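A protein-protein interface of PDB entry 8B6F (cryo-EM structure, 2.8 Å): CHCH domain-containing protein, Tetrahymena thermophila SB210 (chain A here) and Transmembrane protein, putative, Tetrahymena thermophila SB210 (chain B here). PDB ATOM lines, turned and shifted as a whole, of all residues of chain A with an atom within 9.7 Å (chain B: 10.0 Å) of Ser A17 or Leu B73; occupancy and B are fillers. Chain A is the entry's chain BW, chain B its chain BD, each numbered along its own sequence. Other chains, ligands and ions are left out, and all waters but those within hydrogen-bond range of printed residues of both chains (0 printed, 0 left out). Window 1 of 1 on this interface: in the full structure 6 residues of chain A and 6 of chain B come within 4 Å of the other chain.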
ATOM      1  N   TYR A  14       4.293  14.413  -5.359  1.00  0.00           N
ATOM      2  CA  TYR A  14       4.421  14.224  -3.922  1.00  0.00           C
ATOM      3  C   TYR A  14       3.221  14.839  -3.218  1.00  0.00           C
ATOM      4  O   TYR A  14       2.871  15.994  -3.477  1.00  0.00           O
ATOM      5  CB  TYR A  14       5.716  14.854  -3.407  1.00  0.00           C
ATOM      6  CG  TYR A  14       5.921  14.686  -1.921  1.00  0.00           C
ATOM      7  CD1 TYR A  14       6.416  13.499  -1.399  1.00  0.00           C
ATOM      8  CD2 TYR A  14       5.620  15.716  -1.042  1.00  0.00           C
ATOM      9  CE1 TYR A  14       6.602  13.341  -0.043  1.00  0.00           C
ATOM     10  CE2 TYR A  14       5.803  15.569   0.316  1.00  0.00           C
ATOM     11  CZ  TYR A  14       6.294  14.379   0.810  1.00  0.00           C
ATOM     12  OH  TYR A  14       6.480  14.226   2.162  1.00  0.00           O
ATOM     13  N   LYS A  15       2.593  14.065  -2.336  1.00  0.00           N
ATOM     14  CA  LYS A  15       1.443  14.520  -1.567  1.00  0.00           C
ATOM     15  C   LYS A  15       1.903  14.882  -0.161  1.00  0.00           C
ATOM     16  O   LYS A  15       2.464  14.042   0.548  1.00  0.00           O
ATOM     17  CB  LYS A  15       0.360  13.444  -1.519  1.00  0.00           C
ATOM     18  CG  LYS A  15      -0.179  13.058  -2.885  1.00  0.00           C
ATOM     19  CD  LYS A  15      -1.219  11.957  -2.781  1.00  0.00           C
ATOM     20  CE  LYS A  15      -1.784  11.600  -4.146  1.00  0.00           C
ATOM     21  NZ  LYS A  15      -0.729  11.136  -5.091  1.00  0.00           N
ATOM     22  N   TYR A  16       1.659  16.127   0.237  1.00  0.00           N
ATOM     23  CA  TYR A  16       2.116  16.613   1.530  1.00  0.00           C
ATOM     24  C   TYR A  16       1.168  16.171   2.636  1.00  0.00           C
ATOM     25  O   TYR A  16      -0.053  16.155   2.459  1.00  0.00           O
ATOM     26  CB  TYR A  16       2.232  18.137   1.516  1.00  0.00           C
ATOM     27  CG  TYR A  16       3.265  18.659   0.544  1.00  0.00           C
ATOM     28  CD1 TYR A  16       2.955  18.848  -0.796  1.00  0.00           C
ATOM     29  CD2 TYR A  16       4.549  18.967   0.968  1.00  0.00           C
ATOM     30  CE1 TYR A  16       3.896  19.326  -1.687  1.00  0.00           C
ATOM     31  CE2 TYR A  16       5.500  19.444   0.084  1.00  0.00           C
ATOM     32  CZ  TYR A  16       5.166  19.622  -1.240  1.00  0.00           C
ATOM     33  OH  TYR A  16       6.109  20.099  -2.120  1.00  0.00           O
ATOM     34  N   SER A  17       1.740  15.813   3.782  1.00  0.00           N
ATOM     35  CA  SER A  17       0.958  15.359   4.920  1.00  0.00           C
ATOM     36  C   SER A  17       0.425  16.549   5.716  1.00  0.00           C
ATOM     37  O   SER A  17       0.740  17.710   5.443  1.00  0.00           O
ATOM     38  CB  SER A  17       1.797  14.450   5.815  1.00  0.00           C
ATOM     39  OG  SER A  17       2.961  15.116   6.272  1.00  0.00           O
ATOM     40  N   LYS A  18      -0.396  16.244   6.722  1.00  0.00           N
ATOM     41  CA  LYS A  18      -0.978  17.297   7.548  1.00  0.00           C
ATOM     42  C   LYS A  18       0.096  18.067   8.304  1.00  0.00           C
ATOM     43  O   LYS A  18       0.023  19.295   8.419  1.00  0.00           O
ATOM     44  CB  LYS A  18      -1.995  16.697   8.518  1.00  0.00           C
ATOM     45  CG  LYS A  18      -3.202  16.073   7.828  1.00  0.00           C
ATOM     46  CD  LYS A  18      -4.107  15.346   8.813  1.00  0.00           C
ATOM     47  CE  LYS A  18      -4.782  16.297   9.789  1.00  0.00           C
ATOM     48  NZ  LYS A  18      -5.650  17.289   9.096  1.00  0.00           N
ATOM     49  N   GLU A  19       1.105  17.367   8.823  1.00  0.00           N
ATOM     50  CA  GLU A  19       2.190  18.053   9.515  1.00  0.00           C
ATOM     51  C   GLU A  19       2.936  18.986   8.569  1.00  0.00           C
ATOM     52  O   GLU A  19       3.301  20.104   8.947  1.00  0.00           O
ATOM     53  CB  GLU A  19       3.153  17.040  10.134  1.00  0.00           C
ATOM     54  CG  GLU A  19       2.594  16.290  11.333  1.00  0.00           C
ATOM     55  CD  GLU A  19       1.568  15.246  10.949  1.00  0.00           C
ATOM     56  OE1 GLU A  19       1.413  14.979   9.740  1.00  0.00           O
ATOM     57  OE2 GLU A  19       0.916  14.690  11.857  1.00  0.00           O
ATOM     58  N   GLU A  20       3.178  18.540   7.335  1.00  0.00           N
ATOM     59  CA  GLU A  20       3.854  19.392   6.362  1.00  0.00           C
ATOM     60  C   GLU A  20       3.006  20.605   6.004  1.00  0.00           C
ATOM     61  O   GLU A  20       3.536  21.707   5.828  1.00  0.00           O
ATOM     62  CB  GLU A  20       4.199  18.587   5.111  1.00  0.00           C
ATOM     63  CG  GLU A  20       5.331  17.597   5.320  1.00  0.00           C
ATOM     64  CD  GLU A  20       5.649  16.808   4.069  1.00  0.00           C
ATOM     65  OE1 GLU A  20       4.885  16.914   3.088  1.00  0.00           O
ATOM     66  OE2 GLU A  20       6.661  16.080   4.062  1.00  0.00           O
ATOM     67  N   ILE A  21       1.689  20.425   5.885  1.00  0.00           N
ATOM     68  CA  ILE A  21       0.812  21.560   5.610  1.00  0.00           C
ATOM     69  C   ILE A  21       0.877  22.557   6.759  1.00  0.00           C
ATOM     70  O   ILE A  21       0.989  23.769   6.547  1.00  0.00           O
ATOM     71  CB  ILE A  21      -0.628  21.080   5.357  1.00  0.00           C
ATOM     72  CG1 ILE A  21      -0.688  20.237   4.084  1.00  0.00           C
ATOM     73  CG2 ILE A  21      -1.582  22.268   5.250  1.00  0.00           C
ATOM     74  CD1 ILE A  21      -1.986  19.482   3.907  1.00  0.00           C
ATOM     75  N   GLU A  22       0.812  22.058   7.994  1.00  0.00           N
ATOM     76  CA  GLU A  22       0.900  22.939   9.155  1.00  0.00           C
ATOM     77  C   GLU A  22       2.230  23.679   9.181  1.00  0.00           C
ATOM     78  O   GLU A  22       2.278  24.875   9.487  1.00  0.00           O
ATOM     79  CB  GLU A  22       0.708  22.132  10.438  1.00  0.00           C
ATOM     80  CG  GLU A  22      -0.673  21.512  10.568  1.00  0.00           C
ATOM     81  CD  GLU A  22      -0.745  20.480  11.676  1.00  0.00           C
ATOM     82  OE1 GLU A  22       0.277  20.272  12.364  1.00  0.00           O
ATOM     83  OE2 GLU A  22      -1.822  19.874  11.857  1.00  0.00           O
ATOM     84  N   ALA A  23       3.323  22.983   8.867  1.00  0.00           N
ATOM     85  CA  ALA A  23       4.622  23.640   8.785  1.00  0.00           C
ATOM     86  C   ALA A  23       4.597  24.751   7.744  1.00  0.00           C
ATOM     87  O   ALA A  23       4.745  25.932   8.071  1.00  0.00           O
ATOM     88  CB  ALA A  23       5.707  22.614   8.459  1.00  0.00           C
ATOM     89  N   TYR A  24       4.390  24.390   6.478  1.00  0.00           N
ATOM     90  CA  TYR A  24       4.219  25.375   5.411  1.00  0.00           C
ATOM     91  C   TYR A  24       2.773  25.874   5.421  1.00  0.00           C
ATOM     92  O   TYR A  24       2.059  25.817   4.421  1.00  0.00           O
ATOM     93  CB  TYR A  24       4.567  24.772   4.057  1.00  0.00           C
ATOM     94  CG  TYR A  24       5.756  23.841   4.050  1.00  0.00           C
ATOM     95  CD1 TYR A  24       7.039  24.312   4.282  1.00  0.00           C
ATOM     96  CD2 TYR A  24       5.593  22.489   3.781  1.00  0.00           C
ATOM     97  CE1 TYR A  24       8.126  23.460   4.264  1.00  0.00           C
ATOM     98  CE2 TYR A  24       6.670  21.629   3.761  1.00  0.00           C
ATOM     99  CZ  TYR A  24       7.934  22.120   4.002  1.00  0.00           C
ATOM    100  OH  TYR A  24       9.011  21.265   3.981  1.00  0.00           O
ATOM    101  N   GLN A  25       2.352  26.367   6.586  1.00  0.00           N
ATOM    102  CA  GLN A  25       0.954  26.697   6.843  1.00  0.00           C
ATOM    103  C   GLN A  25       0.291  27.318   5.624  1.00  0.00           C
ATOM    104  O   GLN A  25       0.763  28.321   5.080  1.00  0.00           O
ATOM    105  CB  GLN A  25       0.850  27.644   8.046  1.00  0.00           C
ATOM    106  CG  GLN A  25       1.445  29.037   7.863  1.00  0.00           C
ATOM    107  CD  GLN A  25       2.946  29.025   7.679  1.00  0.00           C
ATOM    108  OE1 GLN A  25       3.465  28.365   6.782  1.00  0.00           O
ATOM    109  NE2 GLN A  25       3.655  29.749   8.538  1.00  0.00           N
ATOM    110  N   VAL A  26      -0.801  26.704   5.195  1.00  0.00           N
ATOM    111  CA  VAL A  26      -1.541  27.103   4.001  1.00  0.00           C
ATOM    112  C   VAL A  26      -2.829  27.775   4.455  1.00  0.00           C
ATOM    113  O   VAL A  26      -3.495  27.258   5.359  1.00  0.00           O
ATOM    114  CB  VAL A  26      -1.850  25.896   3.095  1.00  0.00           C
ATOM    115  CG1 VAL A  26      -2.616  26.328   1.855  1.00  0.00           C
ATOM    116  CG2 VAL A  26      -0.567  25.179   2.709  1.00  0.00           C
ATOM    117  N   LYS A  31      -6.466  25.602   1.343  1.00  0.00           N
ATOM    118  CA  LYS A  31      -6.540  24.252   1.888  1.00  0.00           C
ATOM    119  C   LYS A  31      -7.886  23.602   1.598  1.00  0.00           C
ATOM    120  O   LYS A  31      -7.973  22.374   1.496  1.00  0.00           O
ATOM    121  CB  LYS A  31      -6.272  24.282   3.393  1.00  0.00           C
ATOM    122  CG  LYS A  31      -6.159  22.907   4.040  1.00  0.00           C
ATOM    123  CD  LYS A  31      -7.485  22.451   4.631  1.00  0.00           C
ATOM    124  CE  LYS A  31      -7.349  21.099   5.309  1.00  0.00           C
ATOM    125  NZ  LYS A  31      -8.641  20.636   5.888  1.00  0.00           N
ATOM    126  N   VAL A  36      -3.588  21.972  -2.978  1.00  0.00           N
ATOM    127  CA  VAL A  36      -2.586  22.128  -1.931  1.00  0.00           C
ATOM    128  C   VAL A  36      -1.240  21.594  -2.401  1.00  0.00           C
ATOM    129  O   VAL A  36      -0.192  22.194  -2.136  1.00  0.00           O
ATOM    130  CB  VAL A  36      -3.052  21.436  -0.637  1.00  0.00           C
ATOM    131  CG1 VAL A  36      -2.006  21.582   0.458  1.00  0.00           C
ATOM    132  CG2 VAL A  36      -4.383  22.006  -0.181  1.00  0.00           C
ATOM    133  N   ASP A  37      -1.244  20.461  -3.104  1.00  0.00           N
ATOM    134  CA  ASP A  37       0.009  19.859  -3.548  1.00  0.00           C
ATOM    135  C   ASP A  37       0.759  20.777  -4.502  1.00  0.00           C
ATOM    136  O   ASP A  37       1.988  20.875  -4.438  1.00  0.00           O
ATOM    137  CB  ASP A  37      -0.265  18.509  -4.207  1.00  0.00           C
ATOM    138  CG  ASP A  37      -0.860  17.500  -3.243  1.00  0.00           C
ATOM    139  OD1 ASP A  37      -0.506  17.540  -2.046  1.00  0.00           O
ATOM    140  OD2 ASP A  37      -1.681  16.670  -3.684  1.00  0.00           O
ATOM    141  N   ILE A  40       1.873  24.296  -2.369  1.00  0.00           N
ATOM    142  CA  ILE A  40       2.976  24.285  -1.406  1.00  0.00           C
ATOM    143  C   ILE A  40       4.321  24.526  -2.080  1.00  0.00           C
ATOM    144  O   ILE A  40       5.103  25.345  -1.571  1.00  0.00           O
ATOM    145  CB  ILE A  40       2.946  22.982  -0.588  1.00  0.00           C
ATOM    146  CG1 ILE A  40       1.763  23.007   0.383  1.00  0.00           C
ATOM    147  CG2 ILE A  40       4.259  22.785   0.168  1.00  0.00           C
ATOM    148  CD1 ILE A  40       1.523  21.699   1.104  1.00  0.00           C
ATOM    149  N   ILE B  65       1.225  10.246  16.890  1.00  0.00           N
ATOM    150  CA  ILE B  65       1.953   9.982  15.658  1.00  0.00           C
ATOM    151  C   ILE B  65       3.135   9.085  15.997  1.00  0.00           C
ATOM    152  O   ILE B  65       3.531   8.950  17.155  1.00  0.00           O
ATOM    153  CB  ILE B  65       2.429  11.274  14.955  1.00  0.00           C
ATOM    154  CG1 ILE B  65       3.373  12.071  15.861  1.00  0.00           C
ATOM    155  CG2 ILE B  65       1.228  12.117  14.549  1.00  0.00           C
ATOM    156  CD1 ILE B  65       3.939  13.327  15.219  1.00  0.00           C
ATOM    157  N   THR B  66       3.695   8.467  14.964  1.00  0.00           N
ATOM    158  CA  THR B  66       4.733   7.462  15.134  1.00  0.00           C
ATOM    159  C   THR B  66       6.122   8.080  15.048  1.00  0.00           C
ATOM    160  O   THR B  66       6.323   9.131  14.433  1.00  0.00           O
ATOM    161  CB  THR B  66       4.595   6.366  14.077  1.00  0.00           C
ATOM    162  OG1 THR B  66       4.695   6.944  12.769  1.00  0.00           O
ATOM    163  CG2 THR B  66       3.260   5.660  14.219  1.00  0.00           C
ATOM    164  N   ASP B  67       7.088   7.412  15.683  1.00  0.00           N
ATOM    165  CA  ASP B  67       8.475   7.860  15.607  1.00  0.00           C
ATOM    166  C   ASP B  67       9.013   7.769  14.187  1.00  0.00           C
ATOM    167  O   ASP B  67       9.824   8.607  13.776  1.00  0.00           O
ATOM    168  CB  ASP B  67       9.348   7.036  16.554  1.00  0.00           C
ATOM    169  CG  ASP B  67       8.953   7.205  18.006  1.00  0.00           C
ATOM    170  OD1 ASP B  67       8.526   8.318  18.383  1.00  0.00           O
ATOM    171  OD2 ASP B  67       9.068   6.226  18.772  1.00  0.00           O
ATOM    172  N   GLN B  68       8.579   6.765  13.425  1.00  0.00           N
ATOM    173  CA  GLN B  68       8.955   6.698  12.017  1.00  0.00           C
ATOM    174  C   GLN B  68       8.439   7.917  11.265  1.00  0.00           C
ATOM    175  O   GLN B  68       9.141   8.474  10.412  1.00  0.00           O
ATOM    176  CB  GLN B  68       8.424   5.411  11.388  1.00  0.00           C
ATOM    177  CG  GLN B  68       6.907   5.280  11.422  1.00  0.00           C
ATOM    178  CD  GLN B  68       6.420   3.928  10.931  1.00  0.00           C
ATOM    179  OE1 GLN B  68       5.456   3.377  11.462  1.00  0.00           O
ATOM    180  NE2 GLN B  68       7.075   3.392   9.906  1.00  0.00           N
ATOM    181  N   HIS B  69       7.212   8.345  11.566  1.00  0.00           N
ATOM    182  CA  HIS B  69       6.679   9.551  10.943  1.00  0.00           C
ATOM    183  C   HIS B  69       7.476  10.779  11.363  1.00  0.00           C
ATOM    184  O   HIS B  69       7.725  11.674  10.547  1.00  0.00           O
ATOM    185  CB  HIS B  69       5.204   9.714  11.305  1.00  0.00           C
ATOM    186  CG  HIS B  69       4.507  10.784  10.524  1.00  0.00           C
ATOM    187  ND1 HIS B  69       4.602  10.886   9.153  1.00  0.00           N
ATOM    188  CD2 HIS B  69       3.699  11.794  10.922  1.00  0.00           C
ATOM    189  CE1 HIS B  69       3.885  11.915   8.740  1.00  0.00           C
ATOM    190  NE2 HIS B  69       3.327  12.483   9.794  1.00  0.00           N
ATOM    191  N   ARG B  70       7.884  10.844  12.632  1.00  0.00           N
ATOM    192  CA  ARG B  70       8.719  11.955  13.080  1.00  0.00           C
ATOM    193  C   ARG B  70      10.036  11.990  12.316  1.00  0.00           C
ATOM    194  O   ARG B  70      10.485  13.057  11.884  1.00  0.00           O
ATOM    195  CB  ARG B  70       8.984  11.847  14.580  1.00  0.00           C
ATOM    196  CG  ARG B  70       7.772  12.107  15.451  1.00  0.00           C
ATOM    197  CD  ARG B  70       8.158  12.118  16.920  1.00  0.00           C
ATOM    198  NE  ARG B  70       7.026  12.447  17.776  1.00  0.00           N
ATOM    199  CZ  ARG B  70       6.150  11.566  18.239  1.00  0.00           C
ATOM    200  NH1 ARG B  70       6.243  10.279  17.947  1.00  0.00           N
ATOM    201  NH2 ARG B  70       5.154  11.987  19.011  1.00  0.00           N
ATOM    202  N   GLU B  71      10.670  10.829  12.141  1.00  0.00           N
ATOM    203  CA  GLU B  71      11.920  10.776  11.393  1.00  0.00           C
ATOM    204  C   GLU B  71      11.699  11.150   9.934  1.00  0.00           C
ATOM    205  O   GLU B  71      12.545  11.811   9.323  1.00  0.00           O
ATOM    206  CB  GLU B  71      12.539   9.383  11.505  1.00  0.00           C
ATOM    207  CG  GLU B  71      13.011   9.034  12.908  1.00  0.00           C
ATOM    208  CD  GLU B  71      14.139   9.932  13.388  1.00  0.00           C
ATOM    209  OE1 GLU B  71      14.766  10.605  12.544  1.00  0.00           O
ATOM    210  OE2 GLU B  71      14.396   9.967  14.610  1.00  0.00           O
ATOM    211  N   PHE B  72      10.566  10.738   9.360  1.00  0.00           N
ATOM    212  CA  PHE B  72      10.250  11.132   7.992  1.00  0.00           C
ATOM    213  C   PHE B  72      10.134  12.646   7.871  1.00  0.00           C
ATOM    214  O   PHE B  72      10.679  13.245   6.938  1.00  0.00           O
ATOM    215  CB  PHE B  72       8.955  10.458   7.542  1.00  0.00           C
ATOM    216  CG  PHE B  72       8.441  10.956   6.225  1.00  0.00           C
ATOM    217  CD1 PHE B  72       8.999  10.515   5.038  1.00  0.00           C
ATOM    218  CD2 PHE B  72       7.394  11.858   6.172  1.00  0.00           C
ATOM    219  CE1 PHE B  72       8.528  10.969   3.823  1.00  0.00           C
ATOM    220  CE2 PHE B  72       6.917  12.315   4.960  1.00  0.00           C
ATOM    221  CZ  PHE B  72       7.486  11.869   3.784  1.00  0.00           C
ATOM    222  N   LEU B  73       9.441  13.283   8.816  1.00  0.00           N
ATOM    223  CA  LEU B  73       9.336  14.738   8.799  1.00  0.00           C
ATOM    224  C   LEU B  73      10.704  15.386   8.965  1.00  0.00           C
ATOM    225  O   LEU B  73      11.012  16.383   8.303  1.00  0.00           O
ATOM    226  CB  LEU B  73       8.383  15.211   9.896  1.00  0.00           C
ATOM    227  CG  LEU B  73       6.928  14.753   9.774  1.00  0.00           C
ATOM    228  CD1 LEU B  73       6.133  15.228  10.976  1.00  0.00           C
ATOM    229  CD2 LEU B  73       6.291  15.239   8.483  1.00  0.00           C
ATOM    230  N   LYS B  74      11.536  14.837   9.851  1.00  0.00           N
ATOM    231  CA  LYS B  74      12.874  15.384  10.044  1.00  0.00           C
ATOM    232  C   LYS B  74      13.679  15.320   8.754  1.00  0.00           C
ATOM    233  O   LYS B  74      14.371  16.279   8.396  1.00  0.00           O
ATOM    234  CB  LYS B  74      13.588  14.634  11.168  1.00  0.00           C
ATOM    235  CG  LYS B  74      14.953  15.199  11.515  1.00  0.00           C
ATOM    236  CD  LYS B  74      15.538  14.514  12.737  1.00  0.00           C
ATOM    237  CE  LYS B  74      16.863  15.147  13.136  1.00  0.00           C
ATOM    238  NZ  LYS B  74      17.419  14.550  14.384  1.00  0.00           N
ATOM    239  N   LYS B  75      13.598  14.196   8.038  1.00  0.00           N
ATOM    240  CA  LYS B  75      14.268  14.093   6.746  1.00  0.00           C
ATOM    241  C   LYS B  75      13.697  15.097   5.753  1.00  0.00           C
ATOM    242  O   LYS B  75      14.445  15.720   4.990  1.00  0.00           O
ATOM    243  CB  LYS B  75      14.145  12.671   6.202  1.00  0.00           C
ATOM    244  CG  LYS B  75      14.946  11.641   6.984  1.00  0.00           C
ATOM    245  CD  LYS B  75      14.853  10.265   6.343  1.00  0.00           C
ATOM    246  CE  LYS B  75      15.655   9.237   7.126  1.00  0.00           C
ATOM    247  NZ  LYS B  75      15.583   7.883   6.507  1.00  0.00           N
ATOM    248  N   GLN B  76      12.374  15.266   5.744  1.00  0.00           N
ATOM    249  CA  GLN B  76      11.761  16.248   4.856  1.00  0.00           C
ATOM    250  C   GLN B  76      12.246  17.659   5.160  1.00  0.00           C
ATOM    251  O   GLN B  76      12.231  18.522   4.276  1.00  0.00           O
ATOM    252  CB  GLN B  76      10.238  16.178   4.968  1.00  0.00           C
ATOM    253  CG  GLN B  76       9.632  14.907   4.387  1.00  0.00           C
ATOM    254  CD  GLN B  76       9.881  14.759   2.898  1.00  0.00           C
ATOM    255  OE1 GLN B  76      10.179  13.667   2.416  1.00  0.00           O
ATOM    256  NE2 GLN B  76       9.755  15.857   2.160  1.00  0.00           N
ATOM    257  N   GLY B  77      12.675  17.914   6.391  1.00  0.00           N
ATOM    258  CA  GLY B  77      13.262  19.185   6.759  1.00  0.00           C
ATOM    259  C   GLY B  77      12.464  20.012   7.743  1.00  0.00           C
ATOM    260  O   GLY B  77      12.853  21.151   8.021  1.00  0.00           O
ATOM    261  N   LEU B  78      11.362  19.487   8.272  1.00  0.00           N
ATOM    262  CA  LEU B  78      10.608  20.214   9.277  1.00  0.00           C
ATOM    263  C   LEU B  78      11.335  20.172  10.615  1.00  0.00           C
ATOM    264  O   LEU B  78      12.249  19.375  10.835  1.00  0.00           O
ATOM    265  CB  LEU B  78       9.208  19.625   9.428  1.00  0.00           C
ATOM    266  CG  LEU B  78       8.417  19.438   8.133  1.00  0.00           C
ATOM    267  CD1 LEU B  78       6.998  19.029   8.460  1.00  0.00           C
ATOM    268  CD2 LEU B  78       8.438  20.693   7.279  1.00  0.00           C
ATOM    269  N   LYS B  79      10.911  21.049  11.520  1.00  0.00           N
ATOM    270  CA  LYS B  79      11.492  21.143  12.848  1.00  0.00           C
ATOM    271  C   LYS B  79      10.385  21.099  13.890  1.00  0.00           C
ATOM    272  O   LYS B  79       9.261  21.543  13.645  1.00  0.00           O
ATOM    273  CB  LYS B  79      12.319  22.423  13.002  1.00  0.00           C
ATOM    274  CG  LYS B  79      13.499  22.491  12.047  1.00  0.00           C
ATOM    275  CD  LYS B  79      14.284  23.777  12.219  1.00  0.00           C
ATOM    276  CE  LYS B  79      15.479  23.815  11.279  1.00  0.00           C
ATOM    277  NZ  LYS B  79      16.264  25.074  11.426  1.00  0.00           N
ATOM    278  N   VAL B  80      10.713  20.545  15.052  1.00  0.00           N
ATOM    279  CA  VAL B  80       9.747  20.405  16.135  1.00  0.00           C
ATOM    280  C   VAL B  80       9.686  21.720  16.899  1.00  0.00           C
ATOM    281  O   VAL B  80      10.710  22.221  17.372  1.00  0.00           O
ATOM    282  CB  VAL B  80      10.122  19.242  17.064  1.00  0.00           C
ATOM    283  CG1 VAL B  80       9.040  19.029  18.112  1.00  0.00           C
ATOM    284  CG2 VAL B  80      10.347  17.972  16.266  1.00  0.00           C
ATOM    285  N   TYR B  81       8.487  22.281  17.021  1.00  0.00           N
ATOM    286  CA  TYR B  81       8.327  23.519  17.768  1.00  0.00           C
ATOM    287  C   TYR B  81       8.777  23.327  19.208  1.00  0.00           C
ATOM    288  O   TYR B  81       8.380  22.367  19.874  1.00  0.00           O
ATOM    289  CB  TYR B  81       6.869  23.972  17.726  1.00  0.00           C
ATOM    290  CG  TYR B  81       6.587  25.192  18.565  1.00  0.00           C
ATOM    291  CD1 TYR B  81       6.920  26.461  18.116  1.00  0.00           C
ATOM    292  CD2 TYR B  81       5.978  25.075  19.807  1.00  0.00           C
ATOM    293  CE1 TYR B  81       6.659  27.579  18.881  1.00  0.00           C
ATOM    294  CE2 TYR B  81       5.713  26.186  20.579  1.00  0.00           C
ATOM    295  CZ  TYR B  81       6.055  27.435  20.111  1.00  0.00           C
ATOM    296  OH  TYR B  81       5.792  28.545  20.878  1.00  0.00           O
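NE2 of His B69 sits at hydrogen-bond distance from OE1 of Glu A19 (3.1 Å).
O of Ile B65 sits at hydrogen-bond distance from NH1 of Arg B70, 3.1 Å away. The side-chain hydroxyl of Thr B66 lies within hydrogen-bond range of the backbone NH of His B69, 3.1 Å away. The backbone NH (N) of Leu B78 is in hydrogen-bond range of the backbone carbonyl oxygen (O) of Leu B73 (3.1 Å). The side-chain carboxylate of Glu A20 lies within hydrogen-bond range of the side-chain hydroxyl of Tyr A14. The side-chain carboxylate (OE1) of Glu A20 sits at hydrogen-bond distance from the backbone NH (N) of Ser A17 (3.4 Å). The backbone carbonyl oxygen (O) of Ala A23 sits close to the side-chain amide oxygen (OE1) of Gln A25 (3.0 Å).
Tyr A14 touches Phe B72 (OH to CZ, 3.0 Å). Tyr A14 touches Gln B76 (OH to CD, 3.5 Å). Leu B73 touches Ser A17. Ile B65 touches Glu A19 (CG2 to OE2, 3.7 Å). Glu A19 touches Leu B73 (CB to CD1, 3.6 Å). Leu B78 touches Glu A19. Phe B72 touches Glu A20. OE2 of Glu A20 touches CG of Gln B76, 3.2 Å away. Leu B78 touches Ala A23. OH of Tyr A24 touches CD2 of Leu B78 (3.4 Å).
Of the printed residues of chain B, Ser A17 touches Leu B73. Printed residues of chain A within 4 Å of Leu B73: Ser A17 (3.999 Å) and Glu A19 (3.6 Å). Of the printed residues of chain B, Glu A20 touches Phe B72 (3.9 Å), Gln B76 (3.2 Å) and Leu B78 (3.8 Å). Printed residues of chain A within 4 Å of Phe B72: Tyr A14 and Glu A20. No residue of chain A comes within 4 Å of Gly B77. Leu B78 touches four residues of chain A. Of the printed residues of chain A, Ile B65 touches Glu A19 (3.7 Å). Of the printed residues of chain B, Tyr A14 touches Phe B72 and Gln B76. Of the printed residues of chain A, His B69 touches Glu A19. Printed residues of chain B within 4 Å of Ala A23: Leu B78 (3.5 Å). Printed residues of chain B within 4 Å of Tyr A24: Leu B78 (3.4 Å). The nearest printed residue of chain B that does not touch Ser A17 is His B69 (4.1 Å).
Printed residues of chain B that touch a printed residue of chain A: Ile B65, His B69, Phe B72, Leu B73, Gln B76 and Leu B78. Of the 17 printed residues of chain A, 6 touch a printed residue of chain B. Printed residues of chain A that touch a printed residue of chain B: Tyr A14, Ser A17, Glu A19, Glu A20, Ala A23 and Tyr A24. Hydrophobic or aromatic side chains of chain A that line the printed part of chain B: Tyr A14, Ala A23 and Tyr A24. Along chain A the printed residues that touch a printed residue of chain B span positions 14 to 24. Among the printed residues, no Asp or Glu carboxylate lies within 4 Å of a Lys or Arg side-chain nitrogen of the other chain.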
